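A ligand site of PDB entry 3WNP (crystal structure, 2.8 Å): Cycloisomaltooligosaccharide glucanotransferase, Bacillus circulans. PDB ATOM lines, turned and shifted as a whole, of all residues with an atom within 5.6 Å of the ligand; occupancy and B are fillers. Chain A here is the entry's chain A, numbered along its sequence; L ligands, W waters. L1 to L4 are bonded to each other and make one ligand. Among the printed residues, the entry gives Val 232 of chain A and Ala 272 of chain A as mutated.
Merely in contact with the ligand: Tyr 545 (3.3 Å), Met 149 (3.5 Å), Tyr 546 (3.5 Å), Ala 272 (3.5 Å), Phe 465 (3.6 Å), Phe 171 (3.6 Å), Met 199 (3.7 Å), Asp 476 (3.8 Å), Tyr 376 (3.8 Å) and Leu 239 (3.998 Å). 20 residues have an atom within 4 Å of the ligand: Tyr 146, Asp 147, Met 149, His 152, Phe 171, Tyr 197, Met 199, Leu 239, Ala 272, Gln 273, Asn 318, Glu 344, Tyr 376, Phe 465, Asp 476, His 543, Glu 544, Tyr 545, Tyr 546 and Asn 548. The nearest printed residue that does not touch the ligand is Leu 170 (4.1 Å).
The backbone carbonyl oxygen (O) of Glu 544 sits at hydrogen-bond distance from an oxygen (O3) of LIG L1, 2.5 Å away. The side-chain carboxylate (OE2) of Glu 544 sits close to an oxygen (O2) of LG3 L3, at 3.5 Å. An oxygen (O1) of LG2 L2 sits at hydrogen-bond distance from a ring nitrogen (NE2) of His 152, 2.6 Å away. The side-chain carboxylate of Asp 147 lies within hydrogen-bond range of an oxygen (O3) of LG2 L2, at 2.6 Å. The side-chain hydroxyl (OH) of Tyr 146 sits at hydrogen-bond distance from an oxygen (O3) of LG2 L2 (2.6 Å). The side-chain hydroxyl (OH) of Tyr 197 is in hydrogen-bond range of an oxygen (O1) of LG2 L2 (2.8 Å). An oxygen (O1) of LIG L1 sits at hydrogen-bond distance from the backbone carbonyl oxygen of Gln 273, 2.9 Å away. ND2 of Asn 548 sits at hydrogen-bond distance from O1 of LG4 L4, 3.0 Å away. ND2 of Asn 318 lies within hydrogen-bond range of O1 of LIG L1 (3.1 Å). An oxygen (O2) of LIG L1 sits at hydrogen-bond distance from the side-chain carboxylate of Glu 344. A ring nitrogen (ND1) of His 543 sits at hydrogen-bond distance from an oxygen (O1) of LG4 L4 (3.3 Å).
The backbone carbonyl oxygen of Glu 544 sits at hydrogen-bond distance from the side-chain hydroxyl of Tyr 146 (3.4 Å). OE1 of Glu 544 lies within hydrogen-bond range of NE2 of His 543. O of Asn 318 is in hydrogen-bond range of NE2 of Gln 273, 3.0 Å away. The backbone NH (N) of Gln 273 sits close to the side-chain sulfur (SD) of Met 199 (3.6 Å). The side-chain carboxylate (OE2) of Glu 344 sits at hydrogen-bond distance from the side-chain hydroxyl (OH) of Tyr 376, at 2.5 Å. ND1 of His 543 is in hydrogen-bond range of N of Tyr 545, at 3.2 Å. OH of Tyr 546 sits at hydrogen-bond distance from OH of Tyr 342 (3.0 Å). OH of Tyr 546 lies within hydrogen-bond range of NE2 of Gln 144.
Water W1 lies within hydrogen-bond range of an oxygen (O5) of LG4 L4 (2.5 Å) and the backbone carbonyl oxygen (O) of Val 232 (2.9 Å).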
ATOM      1  N   GLN A 144      33.412 -21.938  25.552  1.00  0.00           N
ATOM      2  CA  GLN A 144      32.812 -22.150  24.238  1.00  0.00           C
ATOM      3  C   GLN A 144      33.975 -21.961  23.250  1.00  0.00           C
ATOM      4  O   GLN A 144      34.614 -20.909  23.226  1.00  0.00           O
ATOM      5  CB  GLN A 144      31.662 -21.167  23.975  1.00  0.00           C
ATOM      6  CG  GLN A 144      30.900 -21.355  22.660  1.00  0.00           C
ATOM      7  CD  GLN A 144      30.145 -20.105  22.189  1.00  0.00           C
ATOM      8  OE1 GLN A 144      30.127 -19.758  21.001  1.00  0.00           O
ATOM      9  NE2 GLN A 144      29.533 -19.419  23.117  1.00  0.00           N
ATOM     10  N   TYR A 146      34.931 -21.154  19.848  1.00  0.00           N
ATOM     11  CA  TYR A 146      34.291 -20.435  18.733  1.00  0.00           C
ATOM     12  C   TYR A 146      35.081 -20.545  17.457  1.00  0.00           C
ATOM     13  O   TYR A 146      36.241 -20.161  17.395  1.00  0.00           O
ATOM     14  CB  TYR A 146      34.187 -18.932  19.061  1.00  0.00           C
ATOM     15  CG  TYR A 146      33.383 -18.146  18.026  1.00  0.00           C
ATOM     16  CD1 TYR A 146      32.004 -18.025  18.153  1.00  0.00           C
ATOM     17  CD2 TYR A 146      34.000 -17.561  16.922  1.00  0.00           C
ATOM     18  CE1 TYR A 146      31.268 -17.322  17.207  1.00  0.00           C
ATOM     19  CE2 TYR A 146      33.262 -16.872  15.966  1.00  0.00           C
ATOM     20  CZ  TYR A 146      31.893 -16.749  16.129  1.00  0.00           C
ATOM     21  OH  TYR A 146      31.136 -16.070  15.210  1.00  0.00           O
ATOM     22  N   ASP A 147      34.432 -21.031  16.401  1.00  0.00           N
ATOM     23  CA  ASP A 147      35.086 -21.125  15.092  1.00  0.00           C
ATOM     24  C   ASP A 147      36.398 -21.843  15.153  1.00  0.00           C
ATOM     25  O   ASP A 147      37.409 -21.345  14.687  1.00  0.00           O
ATOM     26  CB  ASP A 147      35.294 -19.739  14.498  1.00  0.00           C
ATOM     27  CG  ASP A 147      34.037 -19.191  13.871  1.00  0.00           C
ATOM     28  OD1 ASP A 147      32.965 -19.756  14.169  1.00  0.00           O
ATOM     29  OD2 ASP A 147      34.145 -18.227  13.077  1.00  0.00           O
ATOM     30  N   MET A 149      36.130 -25.030  13.972  1.00  0.00           N
ATOM     31  CA  MET A 149      35.870 -26.060  12.954  1.00  0.00           C
ATOM     32  C   MET A 149      36.412 -25.641  11.622  1.00  0.00           C
ATOM     33  O   MET A 149      36.614 -24.434  11.368  1.00  0.00           O
ATOM     34  CB  MET A 149      34.370 -26.397  12.823  1.00  0.00           C
ATOM     35  CG  MET A 149      33.460 -25.243  12.431  1.00  0.00           C
ATOM     36  SD  MET A 149      33.094 -24.140  13.822  1.00  0.00           S
ATOM     37  CE  MET A 149      32.230 -22.810  12.975  1.00  0.00           C
ATOM     38  N   HIS A 152      31.316 -25.962   8.699  1.00  0.00           N
ATOM     39  CA  HIS A 152      30.167 -26.129   9.583  1.00  0.00           C
ATOM     40  C   HIS A 152      29.560 -27.521   9.482  1.00  0.00           C
ATOM     41  O   HIS A 152      28.887 -27.978  10.400  1.00  0.00           O
ATOM     42  CB  HIS A 152      29.116 -25.074   9.232  1.00  0.00           C
ATOM     43  CG  HIS A 152      29.405 -23.725   9.817  1.00  0.00           C
ATOM     44  ND1 HIS A 152      30.496 -22.968   9.463  1.00  0.00           N
ATOM     45  CD2 HIS A 152      28.766 -23.038  10.789  1.00  0.00           C
ATOM     46  CE1 HIS A 152      30.507 -21.851  10.169  1.00  0.00           C
ATOM     47  NE2 HIS A 152      29.459 -21.864  10.980  1.00  0.00           N
ATOM     48  N   LEU A 170      36.354 -20.354   7.725  1.00  0.00           N
ATOM     49  CA  LEU A 170      35.592 -19.675   6.686  1.00  0.00           C
ATOM     50  C   LEU A 170      35.973 -18.212   6.464  1.00  0.00           C
ATOM     51  O   LEU A 170      35.568 -17.665   5.481  1.00  0.00           O
ATOM     52  CB  LEU A 170      34.100 -19.745   6.972  1.00  0.00           C
ATOM     53  CG  LEU A 170      33.540 -18.694   7.947  1.00  0.00           C
ATOM     54  CD1 LEU A 170      32.016 -18.600   7.890  1.00  0.00           C
ATOM     55  CD2 LEU A 170      33.983 -19.025   9.364  1.00  0.00           C
ATOM     56  N   PHE A 171      36.688 -17.579   7.389  1.00  0.00           N
ATOM     57  CA  PHE A 171      37.338 -16.270   7.106  1.00  0.00           C
ATOM     58  C   PHE A 171      38.843 -16.457   6.874  1.00  0.00           C
ATOM     59  O   PHE A 171      39.655 -15.531   6.997  1.00  0.00           O
ATOM     60  CB  PHE A 171      37.111 -15.301   8.242  1.00  0.00           C
ATOM     61  CG  PHE A 171      35.678 -14.958   8.453  1.00  0.00           C
ATOM     62  CD1 PHE A 171      35.068 -14.000   7.660  1.00  0.00           C
ATOM     63  CD2 PHE A 171      34.954 -15.552   9.474  1.00  0.00           C
ATOM     64  CE1 PHE A 171      33.733 -13.664   7.867  1.00  0.00           C
ATOM     65  CE2 PHE A 171      33.627 -15.220   9.696  1.00  0.00           C
ATOM     66  CZ  PHE A 171      33.012 -14.281   8.880  1.00  0.00           C
ATOM     67  N   TYR A 197      31.413 -25.128  19.538  1.00  0.00           N
ATOM     68  CA  TYR A 197      30.457 -24.422  18.722  1.00  0.00           C
ATOM     69  C   TYR A 197      30.046 -25.265  17.506  1.00  0.00           C
ATOM     70  O   TYR A 197      30.879 -25.887  16.830  1.00  0.00           O
ATOM     71  CB  TYR A 197      31.059 -23.118  18.280  1.00  0.00           C
ATOM     72  CG  TYR A 197      30.163 -22.244  17.426  1.00  0.00           C
ATOM     73  CD1 TYR A 197      30.051 -22.467  16.057  1.00  0.00           C
ATOM     74  CD2 TYR A 197      29.466 -21.153  17.997  1.00  0.00           C
ATOM     75  CE1 TYR A 197      29.231 -21.656  15.272  1.00  0.00           C
ATOM     76  CE2 TYR A 197      28.651 -20.329  17.213  1.00  0.00           C
ATOM     77  CZ  TYR A 197      28.536 -20.596  15.847  1.00  0.00           C
ATOM     78  OH  TYR A 197      27.766 -19.818  15.031  1.00  0.00           O
ATOM     79  N   MET A 199      26.582 -25.165  14.411  1.00  0.00           N
ATOM     80  CA  MET A 199      25.260 -24.642  14.043  1.00  0.00           C
ATOM     81  C   MET A 199      24.303 -25.817  14.116  1.00  0.00           C
ATOM     82  O   MET A 199      24.684 -26.962  13.901  1.00  0.00           O
ATOM     83  CB  MET A 199      25.257 -24.055  12.609  1.00  0.00           C
ATOM     84  CG  MET A 199      25.510 -22.556  12.506  1.00  0.00           C
ATOM     85  SD  MET A 199      24.173 -21.600  13.273  1.00  0.00           S
ATOM     86  CE  MET A 199      24.782 -19.930  13.248  1.00  0.00           C
ATOM     87  N   VAL A 232      28.333 -14.495   3.864  1.00  0.00           N
ATOM     88  CA  VAL A 232      29.377 -14.103   4.814  1.00  0.00           C
ATOM     89  C   VAL A 232      30.153 -12.957   4.220  1.00  0.00           C
ATOM     90  O   VAL A 232      30.765 -12.163   4.948  1.00  0.00           O
ATOM     91  CB  VAL A 232      30.328 -15.243   5.200  1.00  0.00           C
ATOM     92  CG1 VAL A 232      29.542 -16.496   5.565  1.00  0.00           C
ATOM     93  CG2 VAL A 232      31.318 -15.520   4.085  1.00  0.00           C
ATOM     94  N   LEU A 239      26.712 -19.904   4.137  1.00  0.00           N
ATOM     95  CA  LEU A 239      25.998 -20.952   4.886  1.00  0.00           C
ATOM     96  C   LEU A 239      24.611 -21.265   4.289  1.00  0.00           C
ATOM     97  O   LEU A 239      23.835 -20.364   3.998  1.00  0.00           O
ATOM     98  CB  LEU A 239      25.825 -20.526   6.359  1.00  0.00           C
ATOM     99  CG  LEU A 239      27.112 -20.235   7.146  1.00  0.00           C
ATOM    100  CD1 LEU A 239      26.773 -20.003   8.596  1.00  0.00           C
ATOM    101  CD2 LEU A 239      28.150 -21.355   7.013  1.00  0.00           C
ATOM    102  N   HIS A 270      27.958 -26.568  22.071  1.00  0.00           N
ATOM    103  CA  HIS A 270      27.205 -25.315  22.032  1.00  0.00           C
ATOM    104  C   HIS A 270      26.548 -25.192  20.650  1.00  0.00           C
ATOM    105  O   HIS A 270      27.197 -24.823  19.688  1.00  0.00           O
ATOM    106  CB  HIS A 270      28.153 -24.138  22.321  1.00  0.00           C
ATOM    107  CG  HIS A 270      27.470 -22.808  22.344  1.00  0.00           C
ATOM    108  ND1 HIS A 270      27.148 -22.154  23.520  1.00  0.00           N
ATOM    109  CD2 HIS A 270      27.063 -21.988  21.354  1.00  0.00           C
ATOM    110  CE1 HIS A 270      26.571 -21.003  23.247  1.00  0.00           C
ATOM    111  NE2 HIS A 270      26.512 -20.870  21.936  1.00  0.00           N
ATOM    112  N   ALA A 272      24.421 -23.357  17.959  1.00  0.00           N
ATOM    113  CA  ALA A 272      23.959 -22.027  17.605  1.00  0.00           C
ATOM    114  C   ALA A 272      22.894 -22.072  16.534  1.00  0.00           C
ATOM    115  O   ALA A 272      22.546 -23.143  16.004  1.00  0.00           O
ATOM    116  CB  ALA A 272      25.126 -21.181  17.142  1.00  0.00           C
ATOM    117  N   GLN A 273      22.358 -20.870  16.272  1.00  0.00           N
ATOM    118  CA  GLN A 273      21.416 -20.605  15.185  1.00  0.00           C
ATOM    119  C   GLN A 273      21.517 -19.127  14.808  1.00  0.00           C
ATOM    120  O   GLN A 273      22.016 -18.292  15.606  1.00  0.00           O
ATOM    121  CB  GLN A 273      20.004 -20.900  15.591  1.00  0.00           C
ATOM    122  CG  GLN A 273      19.439 -19.965  16.641  1.00  0.00           C
ATOM    123  CD  GLN A 273      17.925 -19.869  16.620  1.00  0.00           C
ATOM    124  OE1 GLN A 273      17.294 -19.921  15.547  1.00  0.00           O
ATOM    125  NE2 GLN A 273      17.330 -19.722  17.785  1.00  0.00           N
ATOM    126  N   MET A 274      21.011 -18.834  13.597  1.00  0.00           N
ATOM    127  CA  MET A 274      20.933 -17.469  13.055  1.00  0.00           C
ATOM    128  C   MET A 274      19.768 -16.676  13.615  1.00  0.00           C
ATOM    129  O   MET A 274      19.685 -15.476  13.423  1.00  0.00           O
ATOM    130  CB  MET A 274      20.799 -17.517  11.540  1.00  0.00           C
ATOM    131  CG  MET A 274      22.006 -18.100  10.833  1.00  0.00           C
ATOM    132  SD  MET A 274      23.520 -17.204  11.223  1.00  0.00           S
ATOM    133  CE  MET A 274      23.120 -15.496  10.832  1.00  0.00           C
ATOM    134  N   ASN A 318      21.419 -21.629  21.532  1.00  0.00           N
ATOM    135  CA  ASN A 318      21.257 -20.194  21.511  1.00  0.00           C
ATOM    136  C   ASN A 318      19.856 -19.739  21.129  1.00  0.00           C
ATOM    137  O   ASN A 318      19.422 -19.901  19.973  1.00  0.00           O
ATOM    138  CB  ASN A 318      22.246 -19.591  20.550  1.00  0.00           C
ATOM    139  CG  ASN A 318      22.313 -18.108  20.711  1.00  0.00           C
ATOM    140  OD1 ASN A 318      21.684 -17.527  21.600  1.00  0.00           O
ATOM    141  ND2 ASN A 318      23.075 -17.476  19.863  1.00  0.00           N
ATOM    142  N   VAL A 320      18.206 -16.828  20.153  1.00  0.00           N
ATOM    143  CA  VAL A 320      18.682 -15.554  19.611  1.00  0.00           C
ATOM    144  C   VAL A 320      17.631 -14.455  19.643  1.00  0.00           C
ATOM    145  O   VAL A 320      16.499 -14.678  19.224  1.00  0.00           O
ATOM    146  CB  VAL A 320      19.070 -15.737  18.152  1.00  0.00           C
ATOM    147  CG1 VAL A 320      19.437 -14.403  17.540  1.00  0.00           C
ATOM    148  CG2 VAL A 320      20.222 -16.696  18.036  1.00  0.00           C
ATOM    149  N   TYR A 342      20.680 -20.635  27.235  1.00  0.00           N
ATOM    150  CA  TYR A 342      21.586 -19.626  26.728  1.00  0.00           C
ATOM    151  C   TYR A 342      20.864 -18.744  25.725  1.00  0.00           C
ATOM    152  O   TYR A 342      20.215 -19.267  24.825  1.00  0.00           O
ATOM    153  CB  TYR A 342      22.736 -20.332  26.055  1.00  0.00           C
ATOM    154  CG  TYR A 342      23.802 -19.441  25.450  1.00  0.00           C
ATOM    155  CD1 TYR A 342      23.630 -18.850  24.198  1.00  0.00           C
ATOM    156  CD2 TYR A 342      25.021 -19.232  26.111  1.00  0.00           C
ATOM    157  CE1 TYR A 342      24.632 -18.072  23.634  1.00  0.00           C
ATOM    158  CE2 TYR A 342      26.031 -18.450  25.549  1.00  0.00           C
ATOM    159  CZ  TYR A 342      25.839 -17.875  24.312  1.00  0.00           C
ATOM    160  OH  TYR A 342      26.856 -17.103  23.744  1.00  0.00           O
ATOM    161  N   GLU A 344      21.206 -14.965  23.332  1.00  0.00           N
ATOM    162  CA  GLU A 344      21.882 -13.784  22.814  1.00  0.00           C
ATOM    163  C   GLU A 344      20.845 -12.665  22.774  1.00  0.00           C
ATOM    164  O   GLU A 344      19.831 -12.762  22.107  1.00  0.00           O
ATOM    165  CB  GLU A 344      22.422 -14.103  21.408  1.00  0.00           C
ATOM    166  CG  GLU A 344      23.120 -12.952  20.696  1.00  0.00           C
ATOM    167  CD  GLU A 344      23.816 -13.398  19.419  1.00  0.00           C
ATOM    168  OE1 GLU A 344      23.169 -13.943  18.511  1.00  0.00           O
ATOM    169  OE2 GLU A 344      25.032 -13.169  19.310  1.00  0.00           O
ATOM    170  N   TYR A 376      26.432  -8.194  24.252  1.00  0.00           N
ATOM    171  CA  TYR A 376      27.711  -7.550  23.983  1.00  0.00           C
ATOM    172  C   TYR A 376      27.713  -6.084  24.390  1.00  0.00           C
ATOM    173  O   TYR A 376      27.056  -5.274  23.777  1.00  0.00           O
ATOM    174  CB  TYR A 376      28.096  -7.702  22.521  1.00  0.00           C
ATOM    175  CG  TYR A 376      27.821  -9.082  22.009  1.00  0.00           C
ATOM    176  CD1 TYR A 376      28.432 -10.183  22.592  1.00  0.00           C
ATOM    177  CD2 TYR A 376      26.925  -9.315  20.981  1.00  0.00           C
ATOM    178  CE1 TYR A 376      28.151 -11.466  22.164  1.00  0.00           C
ATOM    179  CE2 TYR A 376      26.668 -10.591  20.541  1.00  0.00           C
ATOM    180  CZ  TYR A 376      27.270 -11.667  21.150  1.00  0.00           C
ATOM    181  OH  TYR A 376      27.026 -12.951  20.748  1.00  0.00           O
ATOM    182  N   PHE A 465      35.566  -0.161   4.898  1.00  0.00           N
ATOM    183  CA  PHE A 465      34.412  -0.662   4.121  1.00  0.00           C
ATOM    184  C   PHE A 465      33.674   0.447   3.423  1.00  0.00           C
ATOM    185  O   PHE A 465      33.628   1.579   3.933  1.00  0.00           O
ATOM    186  CB  PHE A 465      33.441  -1.429   5.020  1.00  0.00           C
ATOM    187  CG  PHE A 465      34.111  -2.509   5.807  1.00  0.00           C
ATOM    188  CD1 PHE A 465      34.706  -3.558   5.169  1.00  0.00           C
ATOM    189  CD2 PHE A 465      34.167  -2.439   7.181  1.00  0.00           C
ATOM    190  CE1 PHE A 465      35.350  -4.556   5.884  1.00  0.00           C
ATOM    191  CE2 PHE A 465      34.795  -3.440   7.911  1.00  0.00           C
ATOM    192  CZ  PHE A 465      35.397  -4.490   7.255  1.00  0.00           C
ATOM    193  N   ASP A 476      34.178   0.515  12.614  1.00  0.00           N
ATOM    194  CA  ASP A 476      34.308  -0.948  12.701  1.00  0.00           C
ATOM    195  C   ASP A 476      35.622  -1.471  12.106  1.00  0.00           C
ATOM    196  O   ASP A 476      35.705  -2.587  11.599  1.00  0.00           O
ATOM    197  CB  ASP A 476      33.077  -1.631  12.065  1.00  0.00           C
ATOM    198  CG  ASP A 476      32.922  -1.353  10.561  1.00  0.00           C
ATOM    199  OD1 ASP A 476      33.572  -0.448   9.997  1.00  0.00           O
ATOM    200  OD2 ASP A 476      32.109  -2.082   9.921  1.00  0.00           O
ATOM    201  N   TRP A 478      39.681  -1.652  13.263  1.00  0.00           N
ATOM    202  CA  TRP A 478      40.475  -1.578  14.473  1.00  0.00           C
ATOM    203  C   TRP A 478      41.731  -2.480  14.380  1.00  0.00           C
ATOM    204  O   TRP A 478      41.912  -3.219  13.429  1.00  0.00           O
ATOM    205  CB  TRP A 478      39.596  -2.020  15.632  1.00  0.00           C
ATOM    206  CG  TRP A 478      38.966  -3.333  15.319  1.00  0.00           C
ATOM    207  CD1 TRP A 478      37.789  -3.536  14.663  1.00  0.00           C
ATOM    208  CD2 TRP A 478      39.519  -4.625  15.554  1.00  0.00           C
ATOM    209  NE1 TRP A 478      37.572  -4.870  14.494  1.00  0.00           N
ATOM    210  CE2 TRP A 478      38.631  -5.564  15.025  1.00  0.00           C
ATOM    211  CE3 TRP A 478      40.689  -5.077  16.169  1.00  0.00           C
ATOM    212  CZ2 TRP A 478      38.857  -6.927  15.097  1.00  0.00           C
ATOM    213  CZ3 TRP A 478      40.907  -6.444  16.237  1.00  0.00           C
ATOM    214  CH2 TRP A 478      39.997  -7.346  15.717  1.00  0.00           C
ATOM    215  N   HIS A 543      31.475  -8.212  20.553  1.00  0.00           N
ATOM    216  CA  HIS A 543      30.754  -8.442  19.313  1.00  0.00           C
ATOM    217  C   HIS A 543      30.345  -9.933  19.214  1.00  0.00           C
ATOM    218  O   HIS A 543      30.789 -10.745  20.013  1.00  0.00           O
ATOM    219  CB  HIS A 543      31.642  -8.033  18.139  1.00  0.00           C
ATOM    220  CG  HIS A 543      30.928  -7.892  16.830  1.00  0.00           C
ATOM    221  ND1 HIS A 543      31.019  -8.837  15.822  1.00  0.00           N
ATOM    222  CD2 HIS A 543      30.126  -6.904  16.357  1.00  0.00           C
ATOM    223  CE1 HIS A 543      30.307  -8.435  14.788  1.00  0.00           C
ATOM    224  NE2 HIS A 543      29.751  -7.272  15.083  1.00  0.00           N
ATOM    225  N   GLU A 544      29.498 -10.271  18.259  1.00  0.00           N
ATOM    226  CA  GLU A 544      29.091 -11.660  18.042  1.00  0.00           C
ATOM    227  C   GLU A 544      30.213 -12.493  17.393  1.00  0.00           C
ATOM    228  O   GLU A 544      30.139 -13.715  17.397  1.00  0.00           O
ATOM    229  CB  GLU A 544      27.836 -11.739  17.170  1.00  0.00           C
ATOM    230  CG  GLU A 544      28.028 -11.324  15.712  1.00  0.00           C
ATOM    231  CD  GLU A 544      27.370  -9.987  15.345  1.00  0.00           C
ATOM    232  OE1 GLU A 544      27.315  -9.071  16.186  1.00  0.00           O
ATOM    233  OE2 GLU A 544      26.927  -9.857  14.175  1.00  0.00           O
ATOM    234  N   TYR A 545      31.209 -11.841  16.819  1.00  0.00           N
ATOM    235  CA  TYR A 545      32.323 -12.522  16.216  1.00  0.00           C
ATOM    236  C   TYR A 545      33.419 -12.382  17.267  1.00  0.00           C
ATOM    237  O   TYR A 545      34.049 -11.335  17.447  1.00  0.00           O
ATOM    238  CB  TYR A 545      32.678 -11.945  14.837  1.00  0.00           C
ATOM    239  CG  TYR A 545      33.806 -12.673  14.158  1.00  0.00           C
ATOM    240  CD1 TYR A 545      33.661 -13.961  13.677  1.00  0.00           C
ATOM    241  CD2 TYR A 545      35.047 -12.067  14.019  1.00  0.00           C
ATOM    242  CE1 TYR A 545      34.730 -14.639  13.067  1.00  0.00           C
ATOM    243  CE2 TYR A 545      36.114 -12.722  13.416  1.00  0.00           C
ATOM    244  CZ  TYR A 545      35.958 -13.998  12.951  1.00  0.00           C
ATOM    245  OH  TYR A 545      37.038 -14.623  12.404  1.00  0.00           O
ATOM    246  N   TYR A 546      33.609 -13.479  17.987  1.00  0.00           N
ATOM    247  CA  TYR A 546      34.352 -13.516  19.232  1.00  0.00           C
ATOM    248  C   TYR A 546      35.805 -13.079  19.053  1.00  0.00           C
ATOM    249  O   TYR A 546      36.387 -12.540  19.991  1.00  0.00           O
ATOM    250  CB  TYR A 546      34.299 -14.925  19.846  1.00  0.00           C
ATOM    251  CG  TYR A 546      33.003 -15.367  20.529  1.00  0.00           C
ATOM    252  CD1 TYR A 546      31.790 -14.756  20.291  1.00  0.00           C
ATOM    253  CD2 TYR A 546      33.004 -16.453  21.411  1.00  0.00           C
ATOM    254  CE1 TYR A 546      30.637 -15.176  20.931  1.00  0.00           C
ATOM    255  CE2 TYR A 546      31.850 -16.887  22.041  1.00  0.00           C
ATOM    256  CZ  TYR A 546      30.677 -16.238  21.804  1.00  0.00           C
ATOM    257  OH  TYR A 546      29.528 -16.688  22.405  1.00  0.00           O
ATOM    258  N   ASN A 548      36.781 -10.630  17.600  1.00  0.00           N
ATOM    259  CA  ASN A 548      36.816  -9.199  17.484  1.00  0.00           C
ATOM    260  C   ASN A 548      37.445  -8.663  18.764  1.00  0.00           C
ATOM    261  O   ASN A 548      37.011  -8.985  19.880  1.00  0.00           O
ATOM    262  CB  ASN A 548      35.390  -8.698  17.314  1.00  0.00           C
ATOM    263  CG  ASN A 548      35.279  -7.188  17.208  1.00  0.00           C
ATOM    264  OD1 ASN A 548      35.659  -6.426  18.118  1.00  0.00           O
ATOM    265  ND2 ASN A 548      34.698  -6.742  16.102  1.00  0.00           N
HETATM  266  C1  LIG L   1      26.456 -16.554  17.701  1.00  0.00           C
HETATM  267  C2  LIG L   1      27.488 -15.554  17.179  1.00  0.00           C
HETATM  268  C3  LIG L   1      27.889 -15.903  15.744  1.00  0.00           C
HETATM  269  C4  LIG L   1      26.608 -16.018  14.898  1.00  0.00           C
HETATM  270  C5  LIG L   1      26.830 -16.273  13.414  1.00  0.00           C
HETATM  271  C6  LIG L   1      25.285 -16.661  16.725  1.00  0.00           C
HETATM  272  O1  LIG L   1      24.445 -17.714  17.133  1.00  0.00           O
HETATM  273  O2  LIG L   1      26.032 -16.239  19.045  1.00  0.00           O
HETATM  274  O3  LIG L   1      28.598 -15.580  18.081  1.00  0.00           O
HETATM  275  O4  LIG L   1      28.740 -14.893  15.193  1.00  0.00           O
HETATM  276  O5  LIG L   1      25.764 -17.046  15.453  1.00  0.00           O
HETATM  277  O6  LIG L   1      27.589 -17.456  13.200  1.00  0.00           O
HETATM  278  C1  LG2 L   2      27.985 -17.624  11.830  1.00  0.00           C
HETATM  279  C2  LG2 L   2      28.945 -18.828  11.740  1.00  0.00           C
HETATM  280  C3  LG2 L   2      30.232 -18.522  12.504  1.00  0.00           C
HETATM  281  C4  LG2 L   2      30.824 -17.219  12.026  1.00  0.00           C
HETATM  282  C5  LG2 L   2      29.805 -16.073  12.066  1.00  0.00           C
HETATM  283  C6  LG2 L   2      30.429 -14.850  11.404  1.00  0.00           C
HETATM  284  O1  LG2 L   2      28.398 -19.980  12.350  1.00  0.00           O
HETATM  285  O2  LG2 L   2      31.166 -19.535  12.254  1.00  0.00           O
HETATM  286  O3  LG2 L   2      31.907 -16.882  12.835  1.00  0.00           O
HETATM  287  O4  LG2 L   2      28.651 -16.477  11.322  1.00  0.00           O
HETATM  288  O5  LG2 L   2      29.473 -13.852  11.161  1.00  0.00           O
HETATM  289  C1  LG3 L   3      29.435 -12.822  12.202  1.00  0.00           C
HETATM  290  C2  LG3 L   3      28.221 -11.937  11.957  1.00  0.00           C
HETATM  291  C3  LG3 L   3      28.468 -10.978  10.764  1.00  0.00           C
HETATM  292  C4  LG3 L   3      29.873 -10.351  10.795  1.00  0.00           C
HETATM  293  C5  LG3 L   3      30.894 -11.456  10.999  1.00  0.00           C
HETATM  294  C6  LG3 L   3      32.339 -11.009  11.000  1.00  0.00           C
HETATM  295  O1  LG3 L   3      27.121 -12.800  11.703  1.00  0.00           O
HETATM  296  O2  LG3 L   3      27.464  -9.986  10.741  1.00  0.00           O
HETATM  297  O3  LG3 L   3      30.144  -9.682   9.600  1.00  0.00           O
HETATM  298  O4  LG3 L   3      30.555 -11.958  12.258  1.00  0.00           O
HETATM  299  O5  LG3 L   3      32.413  -9.771  11.653  1.00  0.00           O
HETATM  300  C1  LG4 L   4      33.722  -9.145  11.528  1.00  0.00           C
HETATM  301  C2  LG4 L   4      33.741  -7.935  12.454  1.00  0.00           C
HETATM  302  C3  LG4 L   4      32.672  -6.943  11.973  1.00  0.00           C
HETATM  303  C4  LG4 L   4      32.887  -6.596  10.477  1.00  0.00           C
HETATM  304  C5  LG4 L   4      33.145  -7.837   9.566  1.00  0.00           C
HETATM  305  C6  LG4 L   4      33.627  -7.511   8.134  1.00  0.00           C
HETATM  306  O1  LG4 L   4      33.553  -8.332  13.804  1.00  0.00           O
HETATM  307  O2  LG4 L   4      32.691  -5.774  12.785  1.00  0.00           O
HETATM  308  O3  LG4 L   4      31.787  -5.821  10.018  1.00  0.00           O
HETATM  309  O4  LG4 L   4      34.072  -8.721  10.206  1.00  0.00           O
HETATM  310  O5  LG4 L   4      33.051  -8.298   7.085  1.00  0.00           O
HETATM  311  O   HOH W   1      32.774 -10.087   5.385  1.00  0.00           O
